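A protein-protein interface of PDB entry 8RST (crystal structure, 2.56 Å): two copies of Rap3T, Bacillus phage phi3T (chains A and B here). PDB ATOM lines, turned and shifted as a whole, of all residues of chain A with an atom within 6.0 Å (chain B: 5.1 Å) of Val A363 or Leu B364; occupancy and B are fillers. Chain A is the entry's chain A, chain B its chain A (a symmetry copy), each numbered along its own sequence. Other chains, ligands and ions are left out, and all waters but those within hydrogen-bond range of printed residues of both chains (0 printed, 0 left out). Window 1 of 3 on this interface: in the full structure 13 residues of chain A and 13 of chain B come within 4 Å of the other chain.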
ATOM      1  N   VAL A 336      -6.745  -6.003  10.751  1.00  0.00           N
ATOM      2  CA  VAL A 336      -6.747  -7.459  10.659  1.00  0.00           C
ATOM      3  C   VAL A 336      -5.495  -7.940   9.941  1.00  0.00           C
ATOM      4  O   VAL A 336      -4.858  -8.918  10.352  1.00  0.00           O
ATOM      5  CB  VAL A 336      -8.028  -7.946   9.955  1.00  0.00           C
ATOM      6  CG1 VAL A 336      -7.977  -9.451   9.729  1.00  0.00           C
ATOM      7  CG2 VAL A 336      -9.256  -7.564  10.765  1.00  0.00           C
ATOM      8  N   GLU A 337      -5.113  -7.250   8.863  1.00  0.00           N
ATOM      9  CA  GLU A 337      -3.927  -7.644   8.111  1.00  0.00           C
ATOM     10  C   GLU A 337      -2.656  -7.377   8.908  1.00  0.00           C
ATOM     11  O   GLU A 337      -1.762  -8.228   8.970  1.00  0.00           O
ATOM     12  CB  GLU A 337      -3.883  -6.911   6.771  1.00  0.00           C
ATOM     13  CG  GLU A 337      -2.624  -7.204   5.970  1.00  0.00           C
ATOM     14  CD  GLU A 337      -2.574  -6.459   4.651  1.00  0.00           C
ATOM     15  OE1 GLU A 337      -3.560  -5.773   4.313  1.00  0.00           O
ATOM     16  OE2 GLU A 337      -1.545  -6.564   3.950  1.00  0.00           O
ATOM     17  N   ALA A 340      -2.497  -9.924  11.955  1.00  0.00           N
ATOM     18  CA  ALA A 340      -2.219 -11.280  11.497  1.00  0.00           C
ATOM     19  C   ALA A 340      -0.815 -11.387  10.916  1.00  0.00           C
ATOM     20  O   ALA A 340      -0.184 -12.447  11.003  1.00  0.00           O
ATOM     21  CB  ALA A 340      -3.263 -11.717  10.468  1.00  0.00           C
ATOM     22  N   SER A 341      -0.309 -10.300  10.329  1.00  0.00           N
ATOM     23  CA  SER A 341       1.074 -10.274   9.867  1.00  0.00           C
ATOM     24  C   SER A 341       2.049 -10.280  11.033  1.00  0.00           C
ATOM     25  O   SER A 341       3.138 -10.858  10.927  1.00  0.00           O
ATOM     26  CB  SER A 341       1.308  -9.048   8.983  1.00  0.00           C
ATOM     27  OG  SER A 341       2.686  -8.882   8.686  1.00  0.00           O
ATOM     28  N   ALA A 344       2.105 -13.957  12.181  1.00  0.00           N
ATOM     29  CA  ALA A 344       2.735 -14.862  11.226  1.00  0.00           C
ATOM     30  C   ALA A 344       4.254 -14.769  11.295  1.00  0.00           C
ATOM     31  O   ALA A 344       4.946 -15.793  11.271  1.00  0.00           O
ATOM     32  CB  ALA A 344       2.237 -14.562   9.813  1.00  0.00           C
ATOM     33  N   ALA A 358      -1.382 -20.588   9.186  1.00  0.00           N
ATOM     34  CA  ALA A 358      -2.771 -20.189   9.388  1.00  0.00           C
ATOM     35  C   ALA A 358      -2.924 -18.676   9.472  1.00  0.00           C
ATOM     36  O   ALA A 358      -3.940 -18.131   9.027  1.00  0.00           O
ATOM     37  CB  ALA A 358      -3.327 -20.849  10.649  1.00  0.00           C
ATOM     38  N   TYR A 359      -1.935 -17.979  10.032  1.00  0.00           N
ATOM     39  CA  TYR A 359      -2.023 -16.527  10.115  1.00  0.00           C
ATOM     40  C   TYR A 359      -1.577 -15.855   8.825  1.00  0.00           C
ATOM     41  O   TYR A 359      -2.042 -14.752   8.519  1.00  0.00           O
ATOM     42  CB  TYR A 359      -1.207 -16.019  11.301  1.00  0.00           C
ATOM     43  CG  TYR A 359      -1.879 -16.315  12.617  1.00  0.00           C
ATOM     44  CD1 TYR A 359      -3.247 -16.138  12.770  1.00  0.00           C
ATOM     45  CD2 TYR A 359      -1.157 -16.797  13.699  1.00  0.00           C
ATOM     46  CE1 TYR A 359      -3.876 -16.413  13.966  1.00  0.00           C
ATOM     47  CE2 TYR A 359      -1.779 -17.077  14.902  1.00  0.00           C
ATOM     48  CZ  TYR A 359      -3.137 -16.883  15.028  1.00  0.00           C
ATOM     49  OH  TYR A 359      -3.762 -17.159  16.220  1.00  0.00           O
ATOM     50  N   TYR A 360      -0.691 -16.495   8.060  1.00  0.00           N
ATOM     51  CA  TYR A 360      -0.400 -16.004   6.717  1.00  0.00           C
ATOM     52  C   TYR A 360      -1.622 -16.125   5.819  1.00  0.00           C
ATOM     53  O   TYR A 360      -1.852 -15.274   4.949  1.00  0.00           O
ATOM     54  CB  TYR A 360       0.779 -16.768   6.117  1.00  0.00           C
ATOM     55  CG  TYR A 360       2.129 -16.170   6.439  1.00  0.00           C
ATOM     56  CD1 TYR A 360       2.470 -14.901   5.990  1.00  0.00           C
ATOM     57  CD2 TYR A 360       3.068 -16.880   7.175  1.00  0.00           C
ATOM     58  CE1 TYR A 360       3.703 -14.350   6.276  1.00  0.00           C
ATOM     59  CE2 TYR A 360       4.304 -16.338   7.465  1.00  0.00           C
ATOM     60  CZ  TYR A 360       4.616 -15.074   7.013  1.00  0.00           C
ATOM     61  OH  TYR A 360       5.846 -14.528   7.298  1.00  0.00           O
ATOM     62  N   GLU A 361      -2.415 -17.184   6.009  1.00  0.00           N
ATOM     63  CA  GLU A 361      -3.671 -17.313   5.279  1.00  0.00           C
ATOM     64  C   GLU A 361      -4.633 -16.189   5.642  1.00  0.00           C
ATOM     65  O   GLU A 361      -5.325 -15.647   4.772  1.00  0.00           O
ATOM     66  CB  GLU A 361      -4.315 -18.671   5.563  1.00  0.00           C
ATOM     67  CG  GLU A 361      -3.439 -19.878   5.262  1.00  0.00           C
ATOM     68  CD  GLU A 361      -4.088 -21.188   5.679  1.00  0.00           C
ATOM     69  OE1 GLU A 361      -5.109 -21.570   5.071  1.00  0.00           O
ATOM     70  OE2 GLU A 361      -3.583 -21.836   6.619  1.00  0.00           O
ATOM     71  N   LYS A 362      -4.690 -15.825   6.927  1.00  0.00           N
ATOM     72  CA  LYS A 362      -5.567 -14.738   7.351  1.00  0.00           C
ATOM     73  C   LYS A 362      -5.125 -13.410   6.753  1.00  0.00           C
ATOM     74  O   LYS A 362      -5.959 -12.553   6.431  1.00  0.00           O
ATOM     75  CB  LYS A 362      -5.598 -14.657   8.876  1.00  0.00           C
ATOM     76  CG  LYS A 362      -6.773 -15.386   9.509  1.00  0.00           C
ATOM     77  CD  LYS A 362      -8.082 -14.673   9.213  1.00  0.00           C
ATOM     78  CE  LYS A 362      -9.260 -15.402   9.840  1.00  0.00           C
ATOM     79  NZ  LYS A 362     -10.543 -14.674   9.624  1.00  0.00           N
ATOM     80  N   VAL A 363      -3.814 -13.216   6.598  1.00  0.00           N
ATOM     81  CA  VAL A 363      -3.314 -12.031   5.904  1.00  0.00           C
ATOM     82  C   VAL A 363      -3.808 -12.019   4.464  1.00  0.00           C
ATOM     83  O   VAL A 363      -4.273 -10.993   3.953  1.00  0.00           O
ATOM     84  CB  VAL A 363      -1.776 -11.974   5.966  1.00  0.00           C
ATOM     85  CG1 VAL A 363      -1.250 -10.804   5.151  1.00  0.00           C
ATOM     86  CG2 VAL A 363      -1.301 -11.873   7.405  1.00  0.00           C
ATOM     87  N   LEU A 364      -3.714 -13.167   3.790  1.00  0.00           N
ATOM     88  CA  LEU A 364      -4.205 -13.268   2.421  1.00  0.00           C
ATOM     89  C   LEU A 364      -5.708 -13.031   2.357  1.00  0.00           C
ATOM     90  O   LEU A 364      -6.207 -12.394   1.420  1.00  0.00           O
ATOM     91  CB  LEU A 364      -3.857 -14.641   1.846  1.00  0.00           C
ATOM     92  CG  LEU A 364      -3.106 -14.679   0.516  1.00  0.00           C
ATOM     93  CD1 LEU A 364      -2.971 -16.114   0.040  1.00  0.00           C
ATOM     94  CD2 LEU A 364      -3.809 -13.825  -0.522  1.00  0.00           C
ATOM     95  N   TYR A 365      -6.444 -13.533   3.349  1.00  0.00           N
ATOM     96  CA  TYR A 365      -7.890 -13.338   3.378  1.00  0.00           C
ATOM     97  C   TYR A 365      -8.240 -11.864   3.530  1.00  0.00           C
ATOM     98  O   TYR A 365      -9.117 -11.347   2.830  1.00  0.00           O
ATOM     99  CB  TYR A 365      -8.504 -14.162   4.512  1.00  0.00           C
ATOM    100  CG  TYR A 365      -9.972 -13.887   4.747  1.00  0.00           C
ATOM    101  CD1 TYR A 365     -10.949 -14.539   4.004  1.00  0.00           C
ATOM    102  CD2 TYR A 365     -10.383 -12.978   5.714  1.00  0.00           C
ATOM    103  CE1 TYR A 365     -12.291 -14.289   4.215  1.00  0.00           C
ATOM    104  CE2 TYR A 365     -11.722 -12.722   5.931  1.00  0.00           C
ATOM    105  CZ  TYR A 365     -12.672 -13.380   5.180  1.00  0.00           C
ATOM    106  OH  TYR A 365     -14.008 -13.129   5.394  1.00  0.00           O
ATOM    107  N   ALA A 366      -7.564 -11.169   4.448  1.00  0.00           N
ATOM    108  CA  ALA A 366      -7.867  -9.760   4.674  1.00  0.00           C
ATOM    109  C   ALA A 366      -7.532  -8.917   3.450  1.00  0.00           C
ATOM    110  O   ALA A 366      -8.274  -7.993   3.105  1.00  0.00           O
ATOM    111  CB  ALA A 366      -7.118  -9.249   5.904  1.00  0.00           C
ATOM    112  N   ARG A 367      -6.422  -9.228   2.774  1.00  0.00           N
ATOM    113  CA  ARG A 367      -6.045  -8.465   1.589  1.00  0.00           C
ATOM    114  C   ARG A 367      -7.067  -8.632   0.473  1.00  0.00           C
ATOM    115  O   ARG A 367      -7.375  -7.674  -0.245  1.00  0.00           O
ATOM    116  CB  ARG A 367      -4.656  -8.884   1.110  1.00  0.00           C
ATOM    117  CG  ARG A 367      -3.530  -8.314   1.944  1.00  0.00           C
ATOM    118  CD  ARG A 367      -2.208  -8.361   1.204  1.00  0.00           C
ATOM    119  NE  ARG A 367      -1.362  -7.223   1.545  1.00  0.00           N
ATOM    120  CZ  ARG A 367      -1.081  -6.220   0.724  1.00  0.00           C
ATOM    121  NH1 ARG A 367      -1.517  -6.207  -0.525  1.00  0.00           N
ATOM    122  NH2 ARG A 367      -0.339  -5.208   1.164  1.00  0.00           N
ATOM    123  N   LYS A 368      -7.603  -9.844   0.308  1.00  0.00           N
ATOM    124  CA  LYS A 368      -8.632 -10.060  -0.702  1.00  0.00           C
ATOM    125  C   LYS A 368      -9.908  -9.304  -0.355  1.00  0.00           C
ATOM    126  O   LYS A 368     -10.560  -8.738  -1.240  1.00  0.00           O
ATOM    127  CB  LYS A 368      -8.911 -11.556  -0.852  1.00  0.00           C
ATOM    128  N   TYR B 360       3.642 -19.141   0.646  1.00  0.00           N
ATOM    129  CA  TYR B 360       2.620 -18.177   1.043  1.00  0.00           C
ATOM    130  C   TYR B 360       3.198 -16.771   1.105  1.00  0.00           C
ATOM    131  O   TYR B 360       2.510 -15.792   0.786  1.00  0.00           O
ATOM    132  CB  TYR B 360       2.020 -18.567   2.392  1.00  0.00           C
ATOM    133  CG  TYR B 360       0.843 -19.509   2.294  1.00  0.00           C
ATOM    134  CD1 TYR B 360      -0.330 -19.118   1.664  1.00  0.00           C
ATOM    135  CD2 TYR B 360       0.898 -20.781   2.847  1.00  0.00           C
ATOM    136  CE1 TYR B 360      -1.412 -19.972   1.575  1.00  0.00           C
ATOM    137  CE2 TYR B 360      -0.178 -21.641   2.764  1.00  0.00           C
ATOM    138  CZ  TYR B 360      -1.330 -21.232   2.127  1.00  0.00           C
ATOM    139  OH  TYR B 360      -2.406 -22.083   2.041  1.00  0.00           O
ATOM    140  N   GLU B 361       4.462 -16.650   1.524  1.00  0.00           N
ATOM    141  CA  GLU B 361       5.133 -15.355   1.497  1.00  0.00           C
ATOM    142  C   GLU B 361       5.274 -14.842   0.069  1.00  0.00           C
ATOM    143  O   GLU B 361       5.095 -13.646  -0.190  1.00  0.00           O
ATOM    144  CB  GLU B 361       6.509 -15.455   2.160  1.00  0.00           C
ATOM    145  CG  GLU B 361       6.501 -15.981   3.588  1.00  0.00           C
ATOM    146  CD  GLU B 361       7.902 -16.170   4.146  1.00  0.00           C
ATOM    147  OE1 GLU B 361       8.609 -15.161   4.345  1.00  0.00           O
ATOM    148  OE2 GLU B 361       8.303 -17.329   4.380  1.00  0.00           O
ATOM    149  N   LYS B 362       5.596 -15.735  -0.871  1.00  0.00           N
ATOM    150  CA  LYS B 362       5.723 -15.327  -2.267  1.00  0.00           C
ATOM    151  C   LYS B 362       4.385 -14.868  -2.830  1.00  0.00           C
ATOM    152  O   LYS B 362       4.330 -13.952  -3.661  1.00  0.00           O
ATOM    153  CB  LYS B 362       6.290 -16.477  -3.097  1.00  0.00           C
ATOM    154  CG  LYS B 362       7.796 -16.406  -3.304  1.00  0.00           C
ATOM    155  CD  LYS B 362       8.169 -15.253  -4.220  1.00  0.00           C
ATOM    156  CE  LYS B 362       9.674 -15.176  -4.423  1.00  0.00           C
ATOM    157  NZ  LYS B 362      10.051 -14.097  -5.381  1.00  0.00           N
ATOM    158  N   VAL B 363       3.291 -15.496  -2.393  1.00  0.00           N
ATOM    159  CA  VAL B 363       1.962 -15.026  -2.775  1.00  0.00           C
ATOM    160  C   VAL B 363       1.739 -13.610  -2.264  1.00  0.00           C
ATOM    161  O   VAL B 363       1.250 -12.734  -2.988  1.00  0.00           O
ATOM    162  CB  VAL B 363       0.876 -15.984  -2.251  1.00  0.00           C
ATOM    163  CG1 VAL B 363      -0.510 -15.439  -2.551  1.00  0.00           C
ATOM    164  CG2 VAL B 363       1.044 -17.367  -2.858  1.00  0.00           C
ATOM    165  N   LEU B 364       2.099 -13.366  -1.002  1.00  0.00           N
ATOM    166  CA  LEU B 364       1.969 -12.028  -0.436  1.00  0.00           C
ATOM    167  C   LEU B 364       2.853 -11.032  -1.174  1.00  0.00           C
ATOM    168  O   LEU B 364       2.456  -9.882  -1.399  1.00  0.00           O
ATOM    169  CB  LEU B 364       2.325 -12.057   1.050  1.00  0.00           C
ATOM    170  CG  LEU B 364       1.304 -11.483   2.031  1.00  0.00           C
ATOM    171  CD1 LEU B 364       1.884 -11.473   3.434  1.00  0.00           C
ATOM    172  CD2 LEU B 364       0.881 -10.089   1.608  1.00  0.00           C
ATOM    173  N   TYR B 365       4.056 -11.459  -1.563  1.00  0.00           N
ATOM    174  CA  TYR B 365       4.961 -10.577  -2.291  1.00  0.00           C
ATOM    175  C   TYR B 365       4.383 -10.199  -3.648  1.00  0.00           C
ATOM    176  O   TYR B 365       4.413  -9.028  -4.044  1.00  0.00           O
ATOM    177  CB  TYR B 365       6.326 -11.250  -2.452  1.00  0.00           C
ATOM    178  CG  TYR B 365       7.280 -10.499  -3.354  1.00  0.00           C
ATOM    179  CD1 TYR B 365       8.064  -9.464  -2.860  1.00  0.00           C
ATOM    180  CD2 TYR B 365       7.399 -10.827  -4.699  1.00  0.00           C
ATOM    181  CE1 TYR B 365       8.936  -8.775  -3.682  1.00  0.00           C
ATOM    182  CE2 TYR B 365       8.267 -10.143  -5.527  1.00  0.00           C
ATOM    183  CZ  TYR B 365       9.033  -9.119  -5.013  1.00  0.00           C
ATOM    184  OH  TYR B 365       9.901  -8.436  -5.835  1.00  0.00           O
ATOM    185  N   ALA B 366       3.850 -11.181  -4.378  1.00  0.00           N
ATOM    186  CA  ALA B 366       3.307 -10.900  -5.703  1.00  0.00           C
ATOM    187  C   ALA B 366       2.090  -9.987  -5.620  1.00  0.00           C
ATOM    188  O   ALA B 366       1.921  -9.094  -6.457  1.00  0.00           O
ATOM    189  CB  ALA B 366       2.955 -12.205  -6.418  1.00  0.00           C
ATOM    190  N   ARG B 367       1.237 -10.188  -4.612  1.00  0.00           N
ATOM    191  CA  ARG B 367       0.054  -9.345  -4.471  1.00  0.00           C
ATOM    192  C   ARG B 367       0.435  -7.898  -4.187  1.00  0.00           C
ATOM    193  O   ARG B 367      -0.204  -6.969  -4.695  1.00  0.00           O
ATOM    194  CB  ARG B 367      -0.853  -9.886  -3.367  1.00  0.00           C
ATOM    195  CG  ARG B 367      -1.657 -11.098  -3.785  1.00  0.00           C
ATOM    196  CD  ARG B 367      -2.843 -11.324  -2.866  1.00  0.00           C
ATOM    197  NE  ARG B 367      -3.983 -11.875  -3.590  1.00  0.00           N
ATOM    198  CZ  ARG B 367      -5.101 -11.210  -3.852  1.00  0.00           C
ATOM    199  NH1 ARG B 367      -5.289  -9.977  -3.413  1.00  0.00           N
ATOM    200  NH2 ARG B 367      -6.054 -11.800  -4.567  1.00  0.00           N
ATOM    201  N   LYS B 368       1.471  -7.685  -3.373  1.00  0.00           N
ATOM    202  CA  LYS B 368       1.927  -6.326  -3.105  1.00  0.00           C
ATOM    203  C   LYS B 368       2.501  -5.683  -4.361  1.00  0.00           C
ATOM    204  O   LYS B 368       2.274  -4.495  -4.616  1.00  0.00           O
ATOM    205  CB  LYS B 368       2.961  -6.333  -1.978  1.00  0.00           C
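The side-chain carboxylate (OE2) of Glu A337 lies within salt-bridge range of the guanidinium group (NE) of Arg A367.
CG1 of Val A363 touches CD1 of Leu B364, at 3.6 Å.
Leu A364 touches Val B363 (CD1 to CG1, 3.6 Å).
Arg B367 touches Leu A364 (CD to CD2, 3.6 Å).
CD2 of Leu B364 touches CD of Arg A367, 3.6 Å away.
Printed residues of chain B within 4 Å of Leu A364: Val B363 (3.6 Å) and Arg B367 (3.6 Å).
Of the printed residues of chain B, Arg A367 touches Leu B364 (3.6 Å).
Of the printed residues of chain A, Val B363 touches Leu A364.
Of the printed residues of chain A, Leu B364 touches Val A363 and Arg A367.
Printed residues of chain A within 4 Å of Arg B367: Leu A364 (3.6 Å).
The nearest printed residue of chain B that does not touch Val A363 is Arg B367 (7.0 Å).
The nearest printed residue of chain B that does not touch Leu A364 is Tyr B360 (4.3 Å).
Of the 16 printed residues of chain A, 3 touch a printed residue of chain B.
Hydrophobic or aromatic side chains of chain A that line the printed part of chain B: Val A363 and Leu A364.
Hydrophobic or aromatic side chains of chain B within 4 Å of the printed part of chain A: Val B363 and Leu B364.
Among the printed residues, no Asp or Glu carboxylate lies within 4 Å of a Lys or Arg side-chain nitrogen of the other chain.
Val A363 touches Leu B364, and with the chains exchanged Leu A364 touches Val B363.
Leu A364 touches Arg B367, and with the chains exchanged Arg A367 touches Leu B364.
9 positions are printed for both chains.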
